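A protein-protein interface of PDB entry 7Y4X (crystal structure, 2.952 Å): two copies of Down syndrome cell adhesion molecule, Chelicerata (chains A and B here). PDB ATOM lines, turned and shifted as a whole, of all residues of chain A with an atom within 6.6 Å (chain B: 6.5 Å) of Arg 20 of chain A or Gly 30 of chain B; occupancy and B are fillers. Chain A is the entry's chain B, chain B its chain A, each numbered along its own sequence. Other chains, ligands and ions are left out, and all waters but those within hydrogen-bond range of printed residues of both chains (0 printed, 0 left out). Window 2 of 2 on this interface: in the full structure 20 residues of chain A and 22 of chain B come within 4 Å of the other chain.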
ATOM      1  N   SER A  12      34.533  22.772 -10.984  1.00  0.00           N
ATOM      2  CA  SER A  12      35.482  22.303  -9.986  1.00  0.00           C
ATOM      3  C   SER A  12      36.614  21.530 -10.649  1.00  0.00           C
ATOM      4  O   SER A  12      36.395  20.735 -11.567  1.00  0.00           O
ATOM      5  CB  SER A  12      34.785  21.429  -8.946  1.00  0.00           C
ATOM      6  OG  SER A  12      35.628  21.214  -7.827  1.00  0.00           O
ATOM      7  N   LEU A  15      36.384  17.497  -9.942  1.00  0.00           N
ATOM      8  CA  LEU A  15      35.046  16.986 -10.195  1.00  0.00           C
ATOM      9  C   LEU A  15      35.040  15.464 -10.224  1.00  0.00           C
ATOM     10  O   LEU A  15      35.902  14.836 -10.847  1.00  0.00           O
ATOM     11  CB  LEU A  15      34.513  17.538 -11.516  1.00  0.00           C
ATOM     12  CG  LEU A  15      33.353  18.532 -11.432  1.00  0.00           C
ATOM     13  CD1 LEU A  15      32.838  18.851 -12.822  1.00  0.00           C
ATOM     14  CD2 LEU A  15      32.232  17.991 -10.556  1.00  0.00           C
ATOM     15  N   GLN A  16      34.069  14.875  -9.535  1.00  0.00           N
ATOM     16  CA  GLN A  16      33.811  13.447  -9.596  1.00  0.00           C
ATOM     17  C   GLN A  16      32.344  13.234  -9.931  1.00  0.00           C
ATOM     18  O   GLN A  16      31.494  14.070  -9.615  1.00  0.00           O
ATOM     19  CB  GLN A  16      34.160  12.743  -8.278  1.00  0.00           C
ATOM     20  CG  GLN A  16      35.618  12.871  -7.874  1.00  0.00           C
ATOM     21  CD  GLN A  16      35.798  12.961  -6.374  1.00  0.00           C
ATOM     22  OE1 GLN A  16      35.783  11.948  -5.674  1.00  0.00           O
ATOM     23  NE2 GLN A  16      35.966  14.177  -5.869  1.00  0.00           N
ATOM     24  N   LYS A  18      28.485  11.902 -10.011  1.00  0.00           N
ATOM     25  CA  LYS A  18      27.397  11.957  -9.031  1.00  0.00           C
ATOM     26  C   LYS A  18      27.503  13.153  -8.088  1.00  0.00           C
ATOM     27  O   LYS A  18      26.663  13.288  -7.188  1.00  0.00           O
ATOM     28  CB  LYS A  18      27.267  10.669  -8.199  1.00  0.00           C
ATOM     29  CG  LYS A  18      27.651   9.387  -8.933  1.00  0.00           C
ATOM     30  CD  LYS A  18      26.447   8.740  -9.595  1.00  0.00           C
ATOM     31  CE  LYS A  18      26.874   7.594 -10.504  1.00  0.00           C
ATOM     32  NZ  LYS A  18      27.758   8.056 -11.609  1.00  0.00           N
ATOM     33  N   GLN A  19      28.487  14.033  -8.265  1.00  0.00           N
ATOM     34  CA  GLN A  19      28.536  15.273  -7.508  1.00  0.00           C
ATOM     35  C   GLN A  19      27.646  16.328  -8.162  1.00  0.00           C
ATOM     36  O   GLN A  19      27.222  16.200  -9.314  1.00  0.00           O
ATOM     37  CB  GLN A  19      29.973  15.782  -7.397  1.00  0.00           C
ATOM     38  CG  GLN A  19      30.835  15.037  -6.383  1.00  0.00           C
ATOM     39  CD  GLN A  19      32.251  15.580  -6.310  1.00  0.00           C
ATOM     40  OE1 GLN A  19      32.651  16.416  -7.121  1.00  0.00           O
ATOM     41  NE2 GLN A  19      33.015  15.110  -5.330  1.00  0.00           N
ATOM     42  N   ARG A  20      27.363  17.384  -7.408  1.00  0.00           N
ATOM     43  CA  ARG A  20      26.539  18.487  -7.877  1.00  0.00           C
ATOM     44  C   ARG A  20      27.423  19.640  -8.338  1.00  0.00           C
ATOM     45  O   ARG A  20      28.519  19.852  -7.815  1.00  0.00           O
ATOM     46  CB  ARG A  20      25.589  18.958  -6.773  1.00  0.00           C
ATOM     47  CG  ARG A  20      24.662  17.864  -6.261  1.00  0.00           C
ATOM     48  CD  ARG A  20      23.935  18.276  -4.994  1.00  0.00           C
ATOM     49  NE  ARG A  20      24.836  18.389  -3.851  1.00  0.00           N
ATOM     50  CZ  ARG A  20      24.698  17.701  -2.722  1.00  0.00           C
ATOM     51  NH1 ARG A  20      23.694  16.847  -2.583  1.00  0.00           N
ATOM     52  NH2 ARG A  20      25.564  17.866  -1.731  1.00  0.00           N
ATOM     53  N   GLU A  21      26.938  20.388  -9.326  1.00  0.00           N
ATOM     54  CA  GLU A  21      27.719  21.464  -9.912  1.00  0.00           C
ATOM     55  C   GLU A  21      26.828  22.666 -10.187  1.00  0.00           C
ATOM     56  O   GLU A  21      25.648  22.524 -10.515  1.00  0.00           O
ATOM     57  CB  GLU A  21      28.411  21.007 -11.202  1.00  0.00           C
ATOM     58  CG  GLU A  21      29.435  21.990 -11.725  1.00  0.00           C
ATOM     59  CD  GLU A  21      30.532  22.274 -10.721  1.00  0.00           C
ATOM     60  OE1 GLU A  21      31.178  21.316 -10.250  1.00  0.00           O
ATOM     61  OE2 GLU A  21      30.742  23.462 -10.399  1.00  0.00           O
ATOM     62  N   GLN A  22      27.413  23.853 -10.045  1.00  0.00           N
ATOM     63  CA  GLN A  22      26.718  25.101 -10.329  1.00  0.00           C
ATOM     64  C   GLN A  22      27.723  26.119 -10.843  1.00  0.00           C
ATOM     65  O   GLN A  22      28.815  26.251 -10.285  1.00  0.00           O
ATOM     66  CB  GLN A  22      26.008  25.642  -9.082  1.00  0.00           C
ATOM     67  CG  GLN A  22      25.047  26.787  -9.373  1.00  0.00           C
ATOM     68  CD  GLN A  22      25.628  28.151  -9.032  1.00  0.00           C
ATOM     69  OE1 GLN A  22      26.819  28.401  -9.228  1.00  0.00           O
ATOM     70  NE2 GLN A  22      24.782  29.046  -8.538  1.00  0.00           N
ATOM     71  N   VAL A  64      22.844  24.575 -13.441  1.00  0.00           N
ATOM     72  CA  VAL A  64      22.958  23.621 -12.343  1.00  0.00           C
ATOM     73  C   VAL A  64      22.885  22.202 -12.890  1.00  0.00           C
ATOM     74  O   VAL A  64      22.076  21.908 -13.778  1.00  0.00           O
ATOM     75  CB  VAL A  64      21.858  23.848 -11.282  1.00  0.00           C
ATOM     76  CG1 VAL A  64      21.933  22.791 -10.190  1.00  0.00           C
ATOM     77  CG2 VAL A  64      21.968  25.243 -10.687  1.00  0.00           C
ATOM     78  N   ILE A  65      23.727  21.320 -12.351  1.00  0.00           N
ATOM     79  CA  ILE A  65      23.710  19.897 -12.667  1.00  0.00           C
ATOM     80  C   ILE A  65      23.653  19.125 -11.355  1.00  0.00           C
ATOM     81  O   ILE A  65      24.559  19.248 -10.520  1.00  0.00           O
ATOM     82  CB  ILE A  65      24.933  19.470 -13.496  1.00  0.00           C
ATOM     83  CG1 ILE A  65      24.968  20.228 -14.823  1.00  0.00           C
ATOM     84  CG2 ILE A  65      24.902  17.972 -13.744  1.00  0.00           C
ATOM     85  CD1 ILE A  65      26.290  20.126 -15.549  1.00  0.00           C
ATOM     86  N   LEU A  66      22.601  18.322 -11.180  1.00  0.00           N
ATOM     87  CA  LEU A  66      22.382  17.654  -9.900  1.00  0.00           C
ATOM     88  C   LEU A  66      23.237  16.404  -9.736  1.00  0.00           C
ATOM     89  O   LEU A  66      23.617  16.066  -8.611  1.00  0.00           O
ATOM     90  CB  LEU A  66      20.906  17.294  -9.737  1.00  0.00           C
ATOM     91  CG  LEU A  66      19.882  18.353 -10.147  1.00  0.00           C
ATOM     92  CD1 LEU A  66      18.477  17.816  -9.938  1.00  0.00           C
ATOM     93  CD2 LEU A  66      20.094  19.639  -9.364  1.00  0.00           C
ATOM     94  N   SER A  67      23.548  15.703 -10.826  1.00  0.00           N
ATOM     95  CA  SER A  67      24.383  14.504 -10.752  1.00  0.00           C
ATOM     96  C   SER A  67      25.303  14.498 -11.968  1.00  0.00           C
ATOM     97  O   SER A  67      24.871  14.187 -13.081  1.00  0.00           O
ATOM     98  CB  SER A  67      23.536  13.238 -10.685  1.00  0.00           C
ATOM     99  OG  SER A  67      24.243  12.193 -10.041  1.00  0.00           O
ATOM    100  N   ILE A  68      26.568  14.851 -11.747  1.00  0.00           N
ATOM    101  CA  ILE A  68      27.542  14.880 -12.828  1.00  0.00           C
ATOM    102  C   ILE A  68      27.824  13.459 -13.292  1.00  0.00           C
ATOM    103  O   ILE A  68      28.054  12.556 -12.477  1.00  0.00           O
ATOM    104  CB  ILE A  68      28.832  15.577 -12.371  1.00  0.00           C
ATOM    105  CG1 ILE A  68      28.589  17.075 -12.179  1.00  0.00           C
ATOM    106  CG2 ILE A  68      29.955  15.330 -13.367  1.00  0.00           C
ATOM    107  CD1 ILE A  68      28.545  17.849 -13.479  1.00  0.00           C
ATOM    108  N   THR B   2      27.848  11.101   3.956  1.00  0.00           N
ATOM    109  CA  THR B   2      28.748  11.967   3.202  1.00  0.00           C
ATOM    110  C   THR B   2      28.710  13.364   3.804  1.00  0.00           C
ATOM    111  O   THR B   2      27.650  13.997   3.845  1.00  0.00           O
ATOM    112  CB  THR B   2      28.374  12.004   1.716  1.00  0.00           C
ATOM    113  OG1 THR B   2      27.893  10.716   1.309  1.00  0.00           O
ATOM    114  CG2 THR B   2      29.586  12.377   0.875  1.00  0.00           C
ATOM    115  N   VAL B   3      29.870  13.838   4.252  1.00  0.00           N
ATOM    116  CA  VAL B   3      30.026  15.129   4.921  1.00  0.00           C
ATOM    117  C   VAL B   3      29.997  16.237   3.873  1.00  0.00           C
ATOM    118  O   VAL B   3      30.437  16.018   2.734  1.00  0.00           O
ATOM    119  CB  VAL B   3      31.323  15.141   5.753  1.00  0.00           C
ATOM    120  CG1 VAL B   3      31.898  16.546   5.922  1.00  0.00           C
ATOM    121  CG2 VAL B   3      31.090  14.485   7.106  1.00  0.00           C
ATOM    122  N   PRO B   4      29.468  17.421   4.195  1.00  0.00           N
ATOM    123  CA  PRO B   4      29.428  18.505   3.205  1.00  0.00           C
ATOM    124  C   PRO B   4      30.813  18.885   2.703  1.00  0.00           C
ATOM    125  O   PRO B   4      31.825  18.692   3.382  1.00  0.00           O
ATOM    126  CB  PRO B   4      28.785  19.664   3.976  1.00  0.00           C
ATOM    127  CG  PRO B   4      28.003  19.018   5.059  1.00  0.00           C
ATOM    128  CD  PRO B   4      28.760  17.779   5.437  1.00  0.00           C
ATOM    129  N   GLN B   5      30.843  19.440   1.491  1.00  0.00           N
ATOM    130  CA  GLN B   5      32.068  19.952   0.891  1.00  0.00           C
ATOM    131  C   GLN B   5      31.705  21.123  -0.007  1.00  0.00           C
ATOM    132  O   GLN B   5      30.831  20.996  -0.869  1.00  0.00           O
ATOM    133  CB  GLN B   5      32.800  18.866   0.091  1.00  0.00           C
ATOM    134  CG  GLN B   5      34.242  19.223  -0.242  1.00  0.00           C
ATOM    135  CD  GLN B   5      34.740  18.556  -1.511  1.00  0.00           C
ATOM    136  OE1 GLN B   5      34.724  17.331  -1.631  1.00  0.00           O
ATOM    137  NE2 GLN B   5      35.194  19.364  -2.463  1.00  0.00           N
ATOM    138  N   LYS B   7      32.299  24.004  -2.843  1.00  0.00           N
ATOM    139  CA  LYS B   7      33.067  24.386  -4.019  1.00  0.00           C
ATOM    140  C   LYS B   7      33.535  25.830  -3.864  1.00  0.00           C
ATOM    141  O   LYS B   7      32.725  26.705  -3.540  1.00  0.00           O
ATOM    142  CB  LYS B   7      32.232  24.233  -5.284  1.00  0.00           C
ATOM    143  CG  LYS B   7      32.921  24.730  -6.542  1.00  0.00           C
ATOM    144  CD  LYS B   7      31.961  24.756  -7.715  1.00  0.00           C
ATOM    145  CE  LYS B   7      32.512  25.592  -8.856  1.00  0.00           C
ATOM    146  NZ  LYS B   7      31.458  25.901  -9.864  1.00  0.00           N
ATOM    147  N   LEU B  26      28.248  26.490  -3.030  1.00  0.00           N
ATOM    148  CA  LEU B  26      27.674  25.243  -3.518  1.00  0.00           C
ATOM    149  C   LEU B  26      28.198  24.065  -2.704  1.00  0.00           C
ATOM    150  O   LEU B  26      29.412  23.884  -2.570  1.00  0.00           O
ATOM    151  CB  LEU B  26      27.996  25.047  -4.997  1.00  0.00           C
ATOM    152  CG  LEU B  26      27.795  23.624  -5.538  1.00  0.00           C
ATOM    153  CD1 LEU B  26      26.320  23.273  -5.707  1.00  0.00           C
ATOM    154  CD2 LEU B  26      28.547  23.433  -6.839  1.00  0.00           C
ATOM    155  N   ALA B  27      27.286  23.265  -2.163  1.00  0.00           N
ATOM    156  CA  ALA B  27      27.660  22.004  -1.527  1.00  0.00           C
ATOM    157  C   ALA B  27      27.830  20.974  -2.634  1.00  0.00           C
ATOM    158  O   ALA B  27      26.895  20.258  -3.000  1.00  0.00           O
ATOM    159  CB  ALA B  27      26.610  21.580  -0.509  1.00  0.00           C
ATOM    160  N   ILE B  28      29.047  20.907  -3.178  1.00  0.00           N
ATOM    161  CA  ILE B  28      29.325  19.993  -4.281  1.00  0.00           C
ATOM    162  C   ILE B  28      29.156  18.546  -3.837  1.00  0.00           C
ATOM    163  O   ILE B  28      28.848  17.670  -4.653  1.00  0.00           O
ATOM    164  CB  ILE B  28      30.732  20.271  -4.849  1.00  0.00           C
ATOM    165  CG1 ILE B  28      31.026  19.373  -6.049  1.00  0.00           C
ATOM    166  CG2 ILE B  28      31.796  20.092  -3.779  1.00  0.00           C
ATOM    167  CD1 ILE B  28      32.088  19.920  -6.976  1.00  0.00           C
ATOM    168  N   ALA B  29      29.334  18.270  -2.546  1.00  0.00           N
ATOM    169  CA  ALA B  29      29.073  16.954  -1.987  1.00  0.00           C
ATOM    170  C   ALA B  29      28.443  17.121  -0.612  1.00  0.00           C
ATOM    171  O   ALA B  29      28.672  18.122   0.073  1.00  0.00           O
ATOM    172  CB  ALA B  29      30.352  16.113  -1.887  1.00  0.00           C
ATOM    173  N   GLY B  30      27.638  16.139  -0.218  1.00  0.00           N
ATOM    174  CA  GLY B  30      26.991  16.185   1.079  1.00  0.00           C
ATOM    175  C   GLY B  30      25.544  15.737   1.059  1.00  0.00           C
ATOM    176  O   GLY B  30      24.777  16.120   0.171  1.00  0.00           O
ATOM    177  N   ASP B  31      25.159  14.931   2.041  1.00  0.00           N
ATOM    178  CA  ASP B  31      23.800  14.408   2.073  1.00  0.00           C
ATOM    179  C   ASP B  31      22.833  15.479   2.573  1.00  0.00           C
ATOM    180  O   ASP B  31      23.116  16.158   3.562  1.00  0.00           O
ATOM    181  CB  ASP B  31      23.718  13.179   2.974  1.00  0.00           C
ATOM    182  CG  ASP B  31      24.516  12.007   2.439  1.00  0.00           C
ATOM    183  OD1 ASP B  31      24.660  11.896   1.202  1.00  0.00           O
ATOM    184  OD2 ASP B  31      24.998  11.196   3.256  1.00  0.00           O
ATOM    185  N   PRO B  32      21.697  15.655   1.905  1.00  0.00           N
ATOM    186  CA  PRO B  32      20.669  16.570   2.409  1.00  0.00           C
ATOM    187  C   PRO B  32      20.019  16.009   3.661  1.00  0.00           C
ATOM    188  O   PRO B  32      20.083  14.795   3.906  1.00  0.00           O
ATOM    189  CB  PRO B  32      19.668  16.652   1.245  1.00  0.00           C
ATOM    190  CG  PRO B  32      19.874  15.388   0.482  1.00  0.00           C
ATOM    191  CD  PRO B  32      21.337  15.079   0.598  1.00  0.00           C
ATOM    192  N   LEU B  34      20.734  20.187   3.995  1.00  0.00           N
ATOM    193  CA  LEU B  34      21.906  21.016   4.224  1.00  0.00           C
ATOM    194  C   LEU B  34      21.476  22.383   4.741  1.00  0.00           C
ATOM    195  O   LEU B  34      20.480  22.947   4.278  1.00  0.00           O
ATOM    196  CB  LEU B  34      22.725  21.165   2.939  1.00  0.00           C
ATOM    197  CG  LEU B  34      23.186  19.851   2.300  1.00  0.00           C
ATOM    198  CD1 LEU B  34      23.490  20.046   0.822  1.00  0.00           C
ATOM    199  CD2 LEU B  34      24.400  19.287   3.027  1.00  0.00           C
ATOM    200  N   PHE B  59      20.768  22.790  -1.907  1.00  0.00           N
ATOM    201  CA  PHE B  59      22.172  22.396  -1.864  1.00  0.00           C
ATOM    202  C   PHE B  59      23.129  23.510  -2.278  1.00  0.00           C
ATOM    203  O   PHE B  59      24.318  23.237  -2.484  1.00  0.00           O
ATOM    204  CB  PHE B  59      22.415  21.149  -2.727  1.00  0.00           C
ATOM    205  CG  PHE B  59      22.080  21.335  -4.179  1.00  0.00           C
ATOM    206  CD1 PHE B  59      20.787  21.137  -4.635  1.00  0.00           C
ATOM    207  CD2 PHE B  59      23.059  21.698  -5.089  1.00  0.00           C
ATOM    208  CE1 PHE B  59      20.476  21.305  -5.969  1.00  0.00           C
ATOM    209  CE2 PHE B  59      22.754  21.866  -6.425  1.00  0.00           C
ATOM    210  CZ  PHE B  59      21.461  21.670  -6.865  1.00  0.00           C
ATOM    211  N   ASN B  82      25.255  19.451   7.828  1.00  0.00           N
ATOM    212  CA  ASN B  82      24.255  18.391   7.734  1.00  0.00           C
ATOM    213  C   ASN B  82      24.409  17.490   8.960  1.00  0.00           C
ATOM    214  O   ASN B  82      25.041  17.869   9.948  1.00  0.00           O
ATOM    215  CB  ASN B  82      24.349  17.655   6.379  1.00  0.00           C
ATOM    216  CG  ASN B  82      25.578  16.755   6.249  1.00  0.00           C
ATOM    217  OD1 ASN B  82      26.300  16.496   7.212  1.00  0.00           O
ATOM    218  ND2 ASN B  82      25.811  16.268   5.036  1.00  0.00           N
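Hydrophobic or aromatic side chains of chain A within 4 Å of the printed part of chain B: Val 64 and Leu 66. Hydrophobic or aromatic side chains of chain B that line the printed part of chain A: Leu 26, Ile 28, Leu 34 and Phe 59. Among the printed residues, Asp or Glu carboxylates within 4 Å of a Lys or Arg side-chain nitrogen of the other chain: Glu 21 of chain A with Lys 7 of chain B (2.6 Å).
O of Phe 59 of chain B lies within hydrogen-bond range of N of Ala 27 of chain B (3.0 Å). The backbone NH of Lys 7 of chain B is in hydrogen-bond range of the backbone carbonyl oxygen of Leu 26 of chain B. The side-chain amide nitrogen (NE2) of Gln 16 of chain A sits close to the side-chain amide nitrogen (NE2) of Gln 19 of chain A, 3.1 Å away. The backbone carbonyl oxygen (O) of Gln 19 of chain A lies within hydrogen-bond range of the backbone NH (N) of Ile 68 of chain A (2.9 Å). The backbone carbonyl oxygen (O) of Ala 29 of chain B sits at hydrogen-bond distance from the backbone NH (N) of Gln 5 of chain B, 2.9 Å away. N of Ile 28 of chain B is in hydrogen-bond range of O of Gln 5 of chain B, 2.9 Å away.
Ser 12 of chain A touches Ile 28 of chain B. Leu 26 of chain B touches Arg 20 of chain A. NH2 of Arg 20 of chain A touches C of Ala 29 of chain B (3.2 Å). CD1 of Leu 34 of chain B touches NH2 of Arg 20 of chain A, at 3.9 Å. Arg 20 of chain A touches Phe 59 of chain B (CD to CD2, 3.5 Å). CA of Glu 21 of chain A touches CD2 of Leu 26 of chain B, 3.7 Å away. Glu 21 of chain A touches Ile 28 of chain B. Leu 26 of chain B touches Gln 22 of chain A (CD2 to N, 3.4 Å). CZ of Phe 59 of chain B touches CG1 of Val 64 of chain A (3.5 Å). CZ of Phe 59 of chain B touches CD2 of Leu 66 of chain A, 3.5 Å away.
No position is printed for both chains. Of the 16 pairs that touch across the chains among the printed residues, none has its exchanged pair printed and touching as well.
The backbone carbonyl oxygen of Gly 30 of chain B sits at hydrogen-bond distance from the guanidinium group of Arg 20 of chain A, at 2.7 Å. O of Gln 22 of chain A sits at hydrogen-bond distance from NZ of Lys 7 of chain B, 2.7 Å away. The guanidinium group of Arg 20 of chain A is in hydrogen-bond range of the backbone carbonyl oxygen of Ala 27 of chain B (2.9 Å). The side-chain carboxylate (OE2) of Glu 21 of chain A is in salt-bridge range of the side-chain amino group (NZ) of Lys 7 of chain B (2.6 Å). The backbone carbonyl oxygen (O) of Ile 28 of chain B sits at hydrogen-bond distance from the backbone NH (N) of Arg 20 of chain A (3.1 Å).
Arg 20 of chain A touches just these residues of chain B: Leu 26 (3.7 Å), Ala 27 (2.9 Å), Ile 28 (3.1 Å), Ala 29 (3.2 Å), Gly 30 (2.7 Å), Leu 34 (3.9 Å) and Phe 59 (3.5 Å). Gly 30 of chain B touches just one residue of chain A: Arg 20. Of the printed residues of chain A, Lys 7 of chain B touches Glu 21 and Gln 22. Of the printed residues of chain A, Leu 26 of chain B touches Arg 20, Glu 21 and Gln 22. Of the printed residues of chain A, Ala 29 of chain B touches Arg 20. Printed residues of chain A within 4 Å of Leu 34 of chain B: Arg 20. Printed residues of chain B within 4 Å of Leu 66 of chain A: Phe 59. Gln 16 of chain A touches none of the printed residues of chain B. Asn 82 of chain B touches none of the printed residues of chain A. The nearest residue of chain B that does not touch Arg 20 of chain A is Pro 32 of chain B (4.3 Å). The nearest printed residue of chain A that does not touch Gly 30 of chain B is Gln 19 of chain A (7.0 Å).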
